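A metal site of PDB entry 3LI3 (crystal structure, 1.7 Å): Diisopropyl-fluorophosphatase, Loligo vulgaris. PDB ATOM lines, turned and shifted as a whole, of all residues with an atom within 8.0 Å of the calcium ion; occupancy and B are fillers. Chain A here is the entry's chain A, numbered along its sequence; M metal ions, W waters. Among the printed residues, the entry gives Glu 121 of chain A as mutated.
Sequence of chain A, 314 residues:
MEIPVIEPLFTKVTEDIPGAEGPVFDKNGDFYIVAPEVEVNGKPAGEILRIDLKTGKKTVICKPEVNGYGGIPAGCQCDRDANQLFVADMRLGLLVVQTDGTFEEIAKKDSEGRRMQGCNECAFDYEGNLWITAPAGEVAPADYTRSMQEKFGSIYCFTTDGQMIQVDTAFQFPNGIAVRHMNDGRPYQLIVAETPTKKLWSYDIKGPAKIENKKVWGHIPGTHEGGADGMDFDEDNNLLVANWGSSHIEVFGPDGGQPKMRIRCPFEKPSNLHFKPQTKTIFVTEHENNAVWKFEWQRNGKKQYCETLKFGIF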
ATOM      1  N   GLY A  19     -11.532 -18.803   7.718  1.00  0.00           N
ATOM      2  CA  GLY A  19     -11.687 -19.206   9.106  1.00  0.00           C
ATOM      3  C   GLY A  19     -11.390 -18.120  10.109  1.00  0.00           C
ATOM      4  O   GLY A  19     -11.037 -18.422  11.252  1.00  0.00           O
ATOM      5  N   ALA A  20     -11.532 -16.859   9.683  1.00  0.00           N
ATOM      6  CA  ALA A  20     -11.287 -15.683  10.524  1.00  0.00           C
ATOM      7  C   ALA A  20     -11.497 -15.994  12.002  1.00  0.00           C
ATOM      8  O   ALA A  20     -12.595 -16.325  12.430  1.00  0.00           O
ATOM      9  CB  ALA A  20     -12.185 -14.533  10.091  1.00  0.00           C
ATOM     10  N   GLU A  21     -10.433 -15.842  12.785  1.00  0.00           N
ATOM     11  CA  GLU A  21     -10.470 -16.160  14.193  1.00  0.00           C
ATOM     12  C   GLU A  21      -9.550 -15.290  15.059  1.00  0.00           C
ATOM     13  O   GLU A  21      -8.891 -14.385  14.573  1.00  0.00           O
ATOM     14  CB  GLU A  21     -10.061 -17.626  14.375  1.00  0.00           C
ATOM     15  CG  GLU A  21     -11.224 -18.564  14.623  1.00  0.00           C
ATOM     16  CD  GLU A  21     -11.511 -18.695  16.090  1.00  0.00           C
ATOM     17  OE1 GLU A  21     -11.336 -17.718  16.831  1.00  0.00           O
ATOM     18  OE2 GLU A  21     -11.943 -19.793  16.489  1.00  0.00           O
ATOM     19  N   GLY A  22      -9.557 -15.606  16.357  1.00  0.00           N
ATOM     20  CA  GLY A  22      -8.714 -14.927  17.326  1.00  0.00           C
ATOM     21  C   GLY A  22      -8.466 -13.441  17.241  1.00  0.00           C
ATOM     22  O   GLY A  22      -7.308 -13.024  17.217  1.00  0.00           O
ATOM     23  N   ALA A  74      -5.455 -20.390  15.755  1.00  0.00           N
ATOM     24  CA  ALA A  74      -6.881 -20.171  15.966  1.00  0.00           C
ATOM     25  C   ALA A  74      -7.303 -19.235  17.096  1.00  0.00           C
ATOM     26  O   ALA A  74      -8.450 -18.779  17.104  1.00  0.00           O
ATOM     27  CB  ALA A  74      -7.565 -21.515  16.146  1.00  0.00           C
ATOM     28  N   GLY A  75      -6.425 -18.964  18.047  1.00  0.00           N
ATOM     29  CA  GLY A  75      -6.809 -18.092  19.152  1.00  0.00           C
ATOM     30  C   GLY A  75      -5.652 -17.239  19.627  1.00  0.00           C
ATOM     31  O   GLY A  75      -4.505 -17.680  19.550  1.00  0.00           O
ATOM     32  N   MET A  90      -3.868 -25.214  16.324  1.00  0.00           N
ATOM     33  CA  MET A  90      -4.407 -26.576  16.273  1.00  0.00           C
ATOM     34  C   MET A  90      -3.420 -27.653  15.854  1.00  0.00           C
ATOM     35  O   MET A  90      -3.643 -28.835  16.101  1.00  0.00           O
ATOM     36  CB  MET A  90      -5.633 -26.615  15.348  1.00  0.00           C
ATOM     37  CG  MET A  90      -6.831 -25.819  15.847  1.00  0.00           C
ATOM     38  SD  MET A  90      -7.736 -26.652  17.166  1.00  0.00           S
ATOM     39  CE  MET A  90      -8.899 -27.646  16.206  1.00  0.00           C
ATOM     40  N   CYS A 119      -4.123 -26.737  20.096  1.00  0.00           N
ATOM     41  CA  CYS A 119      -4.955 -25.789  20.844  1.00  0.00           C
ATOM     42  C   CYS A 119      -5.798 -24.879  19.980  1.00  0.00           C
ATOM     43  O   CYS A 119      -5.475 -24.618  18.830  1.00  0.00           O
ATOM     44  CB  CYS A 119      -4.073 -24.947  21.749  1.00  0.00           C
ATOM     45  SG  CYS A 119      -3.143 -25.915  22.957  1.00  0.00           S
ATOM     46  N   ASN A 120      -6.894 -24.369  20.550  1.00  0.00           N
ATOM     47  CA  ASN A 120      -7.759 -23.510  19.768  1.00  0.00           C
ATOM     48  C   ASN A 120      -7.969 -22.103  20.324  1.00  0.00           C
ATOM     49  O   ASN A 120      -8.061 -21.139  19.563  1.00  0.00           O
ATOM     50  CB  ASN A 120      -9.106 -24.196  19.572  1.00  0.00           C
ATOM     51  CG  ASN A 120     -10.004 -23.443  18.619  1.00  0.00           C
ATOM     52  OD1 ASN A 120     -10.652 -22.481  19.009  1.00  0.00           O
ATOM     53  ND2 ASN A 120     -10.014 -23.861  17.367  1.00  0.00           N
ATOM     54  N   GLU A 121      -8.057 -21.983  21.645  1.00  0.00           N
ATOM     55  CA  GLU A 121      -8.309 -20.693  22.266  1.00  0.00           C
ATOM     56  C   GLU A 121      -7.532 -20.567  23.581  1.00  0.00           C
ATOM     57  O   GLU A 121      -7.145 -21.573  24.163  1.00  0.00           O
ATOM     58  CB  GLU A 121      -9.817 -20.548  22.532  1.00  0.00           C
ATOM     59  CG  GLU A 121     -10.252 -19.242  23.204  1.00  0.00           C
ATOM     60  CD  GLU A 121     -10.106 -18.023  22.307  1.00  0.00           C
ATOM     61  OE1 GLU A 121      -8.970 -17.647  21.980  1.00  0.00           O
ATOM     62  OE2 GLU A 121     -11.145 -17.444  21.926  1.00  0.00           O
ATOM     63  N   CYS A 122      -7.268 -19.339  24.005  1.00  0.00           N
ATOM     64  CA  CYS A 122      -6.586 -19.117  25.280  1.00  0.00           C
ATOM     65  C   CYS A 122      -7.066 -17.827  25.927  1.00  0.00           C
ATOM     66  O   CYS A 122      -7.557 -16.930  25.243  1.00  0.00           O
ATOM     67  CB  CYS A 122      -5.065 -19.116  25.115  1.00  0.00           C
ATOM     68  SG  CYS A 122      -4.366 -17.921  23.944  1.00  0.00           S
ATOM     69  N   THR A 133      -7.649 -24.064  25.661  1.00  0.00           N
ATOM     70  CA  THR A 133      -8.489 -25.186  25.262  1.00  0.00           C
ATOM     71  C   THR A 133      -7.754 -25.920  24.144  1.00  0.00           C
ATOM     72  O   THR A 133      -7.162 -25.304  23.260  1.00  0.00           O
ATOM     73  CB  THR A 133      -9.883 -24.760  24.769  1.00  0.00           C
ATOM     74  OG1 THR A 133      -9.745 -23.787  23.722  1.00  0.00           O
ATOM     75  CG2 THR A 133     -10.695 -24.184  25.920  1.00  0.00           C
ATOM     76  N   PRO A 135      -8.835 -28.789  21.603  1.00  0.00           N
ATOM     77  CA  PRO A 135      -9.801 -29.692  20.952  1.00  0.00           C
ATOM     78  C   PRO A 135      -9.198 -30.664  19.943  1.00  0.00           C
ATOM     79  O   PRO A 135      -9.848 -31.629  19.529  1.00  0.00           O
ATOM     80  CB  PRO A 135     -10.796 -28.732  20.334  1.00  0.00           C
ATOM     81  CG  PRO A 135      -9.919 -27.588  19.903  1.00  0.00           C
ATOM     82  CD  PRO A 135      -8.955 -27.420  21.071  1.00  0.00           C
ATOM     83  N   PHE A 173     -14.669 -31.229  21.947  1.00  0.00           N
ATOM     84  CA  PHE A 173     -14.315 -29.978  21.311  1.00  0.00           C
ATOM     85  C   PHE A 173     -14.425 -28.748  22.202  1.00  0.00           C
ATOM     86  O   PHE A 173     -15.300 -27.889  22.025  1.00  0.00           O
ATOM     87  CB  PHE A 173     -15.099 -29.763  20.010  1.00  0.00           C
ATOM     88  CG  PHE A 173     -14.342 -28.988  18.977  1.00  0.00           C
ATOM     89  CD1 PHE A 173     -14.242 -27.603  19.051  1.00  0.00           C
ATOM     90  CD2 PHE A 173     -13.670 -29.641  17.948  1.00  0.00           C
ATOM     91  CE1 PHE A 173     -13.472 -26.891  18.128  1.00  0.00           C
ATOM     92  CE2 PHE A 173     -12.905 -28.953  17.020  1.00  0.00           C
ATOM     93  CZ  PHE A 173     -12.808 -27.566  17.108  1.00  0.00           C
ATOM     94  N   PRO A 174     -13.545 -28.646  23.208  1.00  0.00           N
ATOM     95  CA  PRO A 174     -13.559 -27.493  24.107  1.00  0.00           C
ATOM     96  C   PRO A 174     -13.147 -26.340  23.190  1.00  0.00           C
ATOM     97  O   PRO A 174     -12.259 -26.492  22.354  1.00  0.00           O
ATOM     98  CB  PRO A 174     -12.496 -27.840  25.149  1.00  0.00           C
ATOM     99  CG  PRO A 174     -11.557 -28.755  24.403  1.00  0.00           C
ATOM    100  CD  PRO A 174     -12.516 -29.618  23.614  1.00  0.00           C
ATOM    101  N   ASN A 175     -13.790 -25.192  23.339  1.00  0.00           N
ATOM    102  CA  ASN A 175     -13.515 -24.103  22.430  1.00  0.00           C
ATOM    103  C   ASN A 175     -13.234 -22.783  23.142  1.00  0.00           C
ATOM    104  O   ASN A 175     -12.139 -22.553  23.633  1.00  0.00           O
ATOM    105  CB  ASN A 175     -14.706 -23.978  21.483  1.00  0.00           C
ATOM    106  CG  ASN A 175     -14.316 -23.369  20.173  1.00  0.00           C
ATOM    107  OD1 ASN A 175     -13.417 -22.553  20.130  1.00  0.00           O
ATOM    108  ND2 ASN A 175     -15.008 -23.735  19.103  1.00  0.00           N
ATOM    109  N   GLY A 176     -14.241 -21.907  23.193  1.00  0.00           N
ATOM    110  CA  GLY A 176     -14.042 -20.637  23.868  1.00  0.00           C
ATOM    111  C   GLY A 176     -13.738 -20.860  25.334  1.00  0.00           C
ATOM    112  O   GLY A 176     -14.129 -21.869  25.916  1.00  0.00           O
ATOM    113  N   ILE A 177     -13.019 -19.909  25.917  1.00  0.00           N
ATOM    114  CA  ILE A 177     -12.667 -19.985  27.330  1.00  0.00           C
ATOM    115  C   ILE A 177     -12.554 -18.552  27.845  1.00  0.00           C
ATOM    116  O   ILE A 177     -12.161 -17.644  27.115  1.00  0.00           O
ATOM    117  CB  ILE A 177     -11.338 -20.764  27.524  1.00  0.00           C
ATOM    118  CG1 ILE A 177     -11.063 -20.975  29.017  1.00  0.00           C
ATOM    119  CG2 ILE A 177     -10.183 -20.017  26.865  1.00  0.00           C
ATOM    120  CD1 ILE A 177     -10.016 -22.034  29.301  1.00  0.00           C
ATOM    121  N   THR A 195     -18.372 -26.861  22.254  1.00  0.00           N
ATOM    122  CA  THR A 195     -19.174 -26.559  21.076  1.00  0.00           C
ATOM    123  C   THR A 195     -20.380 -27.406  20.668  1.00  0.00           C
ATOM    124  O   THR A 195     -21.518 -26.956  20.776  1.00  0.00           O
ATOM    125  CB  THR A 195     -18.260 -26.358  19.854  1.00  0.00           C
ATOM    126  OG1 THR A 195     -17.296 -25.346  20.155  1.00  0.00           O
ATOM    127  CG2 THR A 195     -19.075 -25.908  18.643  1.00  0.00           C
ATOM    128  N   ALA A 228     -21.375 -22.794  20.865  1.00  0.00           N
ATOM    129  CA  ALA A 228     -20.492 -21.742  21.382  1.00  0.00           C
ATOM    130  C   ALA A 228     -19.069 -21.846  20.872  1.00  0.00           C
ATOM    131  O   ALA A 228     -18.448 -22.910  20.920  1.00  0.00           O
ATOM    132  CB  ALA A 228     -20.487 -21.757  22.905  1.00  0.00           C
ATOM    133  N   ASP A 229     -18.568 -20.724  20.385  1.00  0.00           N
ATOM    134  CA  ASP A 229     -17.211 -20.658  19.883  1.00  0.00           C
ATOM    135  C   ASP A 229     -16.430 -19.727  20.813  1.00  0.00           C
ATOM    136  O   ASP A 229     -16.010 -20.142  21.894  1.00  0.00           O
ATOM    137  CB  ASP A 229     -17.182 -20.140  18.435  1.00  0.00           C
ATOM    138  CG  ASP A 229     -15.833 -20.320  17.782  1.00  0.00           C
ATOM    139  OD1 ASP A 229     -14.847 -20.339  18.540  1.00  0.00           O
ATOM    140  OD2 ASP A 229     -15.746 -20.435  16.542  1.00  0.00           O
ATOM    141  N   GLY A 230     -16.243 -18.468  20.410  1.00  0.00           N
ATOM    142  CA  GLY A 230     -15.500 -17.518  21.238  1.00  0.00           C
ATOM    143  C   GLY A 230     -16.342 -16.743  22.232  1.00  0.00           C
ATOM    144  O   GLY A 230     -17.545 -16.582  22.038  1.00  0.00           O
ATOM    145  N   MET A 231     -15.704 -16.251  23.291  1.00  0.00           N
ATOM    146  CA  MET A 231     -16.404 -15.495  24.334  1.00  0.00           C
ATOM    147  C   MET A 231     -15.535 -14.454  25.035  1.00  0.00           C
ATOM    148  O   MET A 231     -14.303 -14.550  25.019  1.00  0.00           O
ATOM    149  CB  MET A 231     -16.935 -16.462  25.390  1.00  0.00           C
ATOM    150  CG  MET A 231     -15.824 -17.315  26.009  1.00  0.00           C
ATOM    151  SD  MET A 231     -16.400 -18.480  27.276  1.00  0.00           S
ATOM    152  CE  MET A 231     -17.797 -19.096  26.433  1.00  0.00           C
ATOM    153  N   TRP A 244     -21.888 -20.109  16.938  1.00  0.00           N
ATOM    154  CA  TRP A 244     -21.612 -20.493  15.552  1.00  0.00           C
ATOM    155  C   TRP A 244     -22.756 -21.301  14.933  1.00  0.00           C
ATOM    156  O   TRP A 244     -23.115 -22.375  15.438  1.00  0.00           O
ATOM    157  CB  TRP A 244     -20.322 -21.314  15.519  1.00  0.00           C
ATOM    158  CG  TRP A 244     -19.667 -21.433  14.176  1.00  0.00           C
ATOM    159  CD1 TRP A 244     -18.648 -20.653  13.689  1.00  0.00           C
ATOM    160  CD2 TRP A 244     -19.910 -22.436  13.176  1.00  0.00           C
ATOM    161  NE1 TRP A 244     -18.238 -21.109  12.463  1.00  0.00           N
ATOM    162  CE2 TRP A 244     -18.987 -22.209  12.122  1.00  0.00           C
ATOM    163  CE3 TRP A 244     -20.809 -23.505  13.071  1.00  0.00           C
ATOM    164  CZ2 TRP A 244     -18.948 -23.019  10.986  1.00  0.00           C
ATOM    165  CZ3 TRP A 244     -20.761 -24.304  11.936  1.00  0.00           C
ATOM    166  CH2 TRP A 244     -19.837 -24.062  10.910  1.00  0.00           C
ATOM    167  N   SER A 271     -17.938 -16.379  14.971  1.00  0.00           N
ATOM    168  CA  SER A 271     -16.921 -17.253  15.544  1.00  0.00           C
ATOM    169  C   SER A 271     -16.265 -16.709  16.801  1.00  0.00           C
ATOM    170  O   SER A 271     -16.297 -17.340  17.849  1.00  0.00           O
ATOM    171  CB  SER A 271     -15.847 -17.547  14.492  1.00  0.00           C
ATOM    172  OG  SER A 271     -14.756 -18.245  15.075  1.00  0.00           O
ATOM    173  N   ASN A 272     -15.662 -15.541  16.698  1.00  0.00           N
ATOM    174  CA  ASN A 272     -15.003 -14.984  17.872  1.00  0.00           C
ATOM    175  C   ASN A 272     -15.190 -13.485  17.916  1.00  0.00           C
ATOM    176  O   ASN A 272     -15.637 -12.867  16.952  1.00  0.00           O
ATOM    177  CB  ASN A 272     -13.512 -15.324  17.860  1.00  0.00           C
ATOM    178  CG  ASN A 272     -12.973 -15.612  19.245  1.00  0.00           C
ATOM    179  OD1 ASN A 272     -13.452 -15.056  20.238  1.00  0.00           O
ATOM    180  ND2 ASN A 272     -11.968 -16.477  19.325  1.00  0.00           N
ATOM    181  N   THR A 285     -15.534 -11.927  14.255  1.00  0.00           N
ATOM    182  CA  THR A 285     -15.109 -12.671  13.075  1.00  0.00           C
ATOM    183  C   THR A 285     -16.216 -13.670  12.784  1.00  0.00           C
ATOM    184  O   THR A 285     -16.888 -14.141  13.691  1.00  0.00           O
ATOM    185  CB  THR A 285     -13.798 -13.449  13.316  1.00  0.00           C
ATOM    186  OG1 THR A 285     -13.986 -14.426  14.342  1.00  0.00           O
ATOM    187  CG2 THR A 285     -12.672 -12.510  13.709  1.00  0.00           C
ATOM    188  N   HIS A 287     -17.608 -16.989   9.883  1.00  0.00           N
ATOM    189  CA  HIS A 287     -17.248 -17.917   8.824  1.00  0.00           C
ATOM    190  C   HIS A 287     -18.218 -18.128   7.683  1.00  0.00           C
ATOM    191  O   HIS A 287     -18.061 -19.068   6.902  1.00  0.00           O
ATOM    192  CB  HIS A 287     -16.917 -19.262   9.456  1.00  0.00           C
ATOM    193  CG  HIS A 287     -15.820 -19.190  10.467  1.00  0.00           C
ATOM    194  ND1 HIS A 287     -15.524 -20.216  11.338  1.00  0.00           N
ATOM    195  CD2 HIS A 287     -14.923 -18.204  10.746  1.00  0.00           C
ATOM    196  CE1 HIS A 287     -14.519 -19.861  12.112  1.00  0.00           C
ATOM    197  NE2 HIS A 287     -14.127 -18.653  11.767  1.00  0.00           N
HETATM  198 CA    CA M   1     -12.460 -20.850  18.616  1.00  0.00          CA
HETATM  199  O   HOH W   1     -12.830 -19.509  20.730  1.00  0.00           O
HETATM  200  O   HOH W   2     -10.285 -19.547  19.045  1.00  0.00           O
HETATM  201  O   HOH W   3     -13.511 -22.395  16.746  1.00  0.00           O
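Of the 28 residues printed, 4 come within 4 Å of the calcium ion. The nearest printed residue that does not touch the calcium ion is Asn 272 (4.5 Å).
Water W3 bridges the side-chain carboxylate (OD2) of Asp 229 (3.0 Å) and the side-chain amide nitrogen (ND2) of Asn 175 (3.1 Å). Water W1 lies within hydrogen-bond range of the side-chain carboxylate of Glu 121 (2.9 Å), the backbone carbonyl oxygen of Asp 229 (3.4 Å) and the side-chain amide nitrogen of Asn 272 (3.5 Å).
The calcium ion is bound by the side-chain carboxylate (OE2) of Glu 21 (2.4 Å). The calcium ion is bound by the side-chain carboxylate (OD1) of Asp 229 (2.4 Å). The calcium ion is bound by the side-chain amide oxygen (OD1) of Asn 120. The calcium ion is bound by OD1 of Asn 175, at 2.5 Å. Water W1 is bound to the calcium ion. The calcium ion is bound by water W2 (2.6 Å). Water W3 is bound to the calcium ion, 2.6 Å away.
ND2 of Asn 272 is in hydrogen-bond range of OE1 of Glu 21, 2.9 Å away. The backbone NH (N) of Gly 176 sits at hydrogen-bond distance from the backbone carbonyl oxygen (O) of Asp 229 (2.8 Å). The backbone NH of Asn 120 sits at hydrogen-bond distance from the backbone carbonyl oxygen of Thr 133. The backbone carbonyl oxygen (O) of Asn 175 is in hydrogen-bond range of the side-chain hydroxyl (OG1) of Thr 133, at 2.7 Å. The backbone carbonyl oxygen (O) of Asn 120 sits at hydrogen-bond distance from the backbone NH (N) of Gly 75 (3.1 Å). The side-chain amide nitrogen of Asn 175 is in hydrogen-bond range of the side-chain hydroxyl of Thr 195, at 3.0 Å. The side-chain hydroxyl (OG) of Ser 271 lies within hydrogen-bond range of the side-chain carboxylate (OD2) of Asp 229 (2.8 Å). The side-chain amide nitrogen (ND2) of Asn 120 lies within hydrogen-bond range of the side-chain sulfur (SD) of Met 90, 3.6 Å away.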
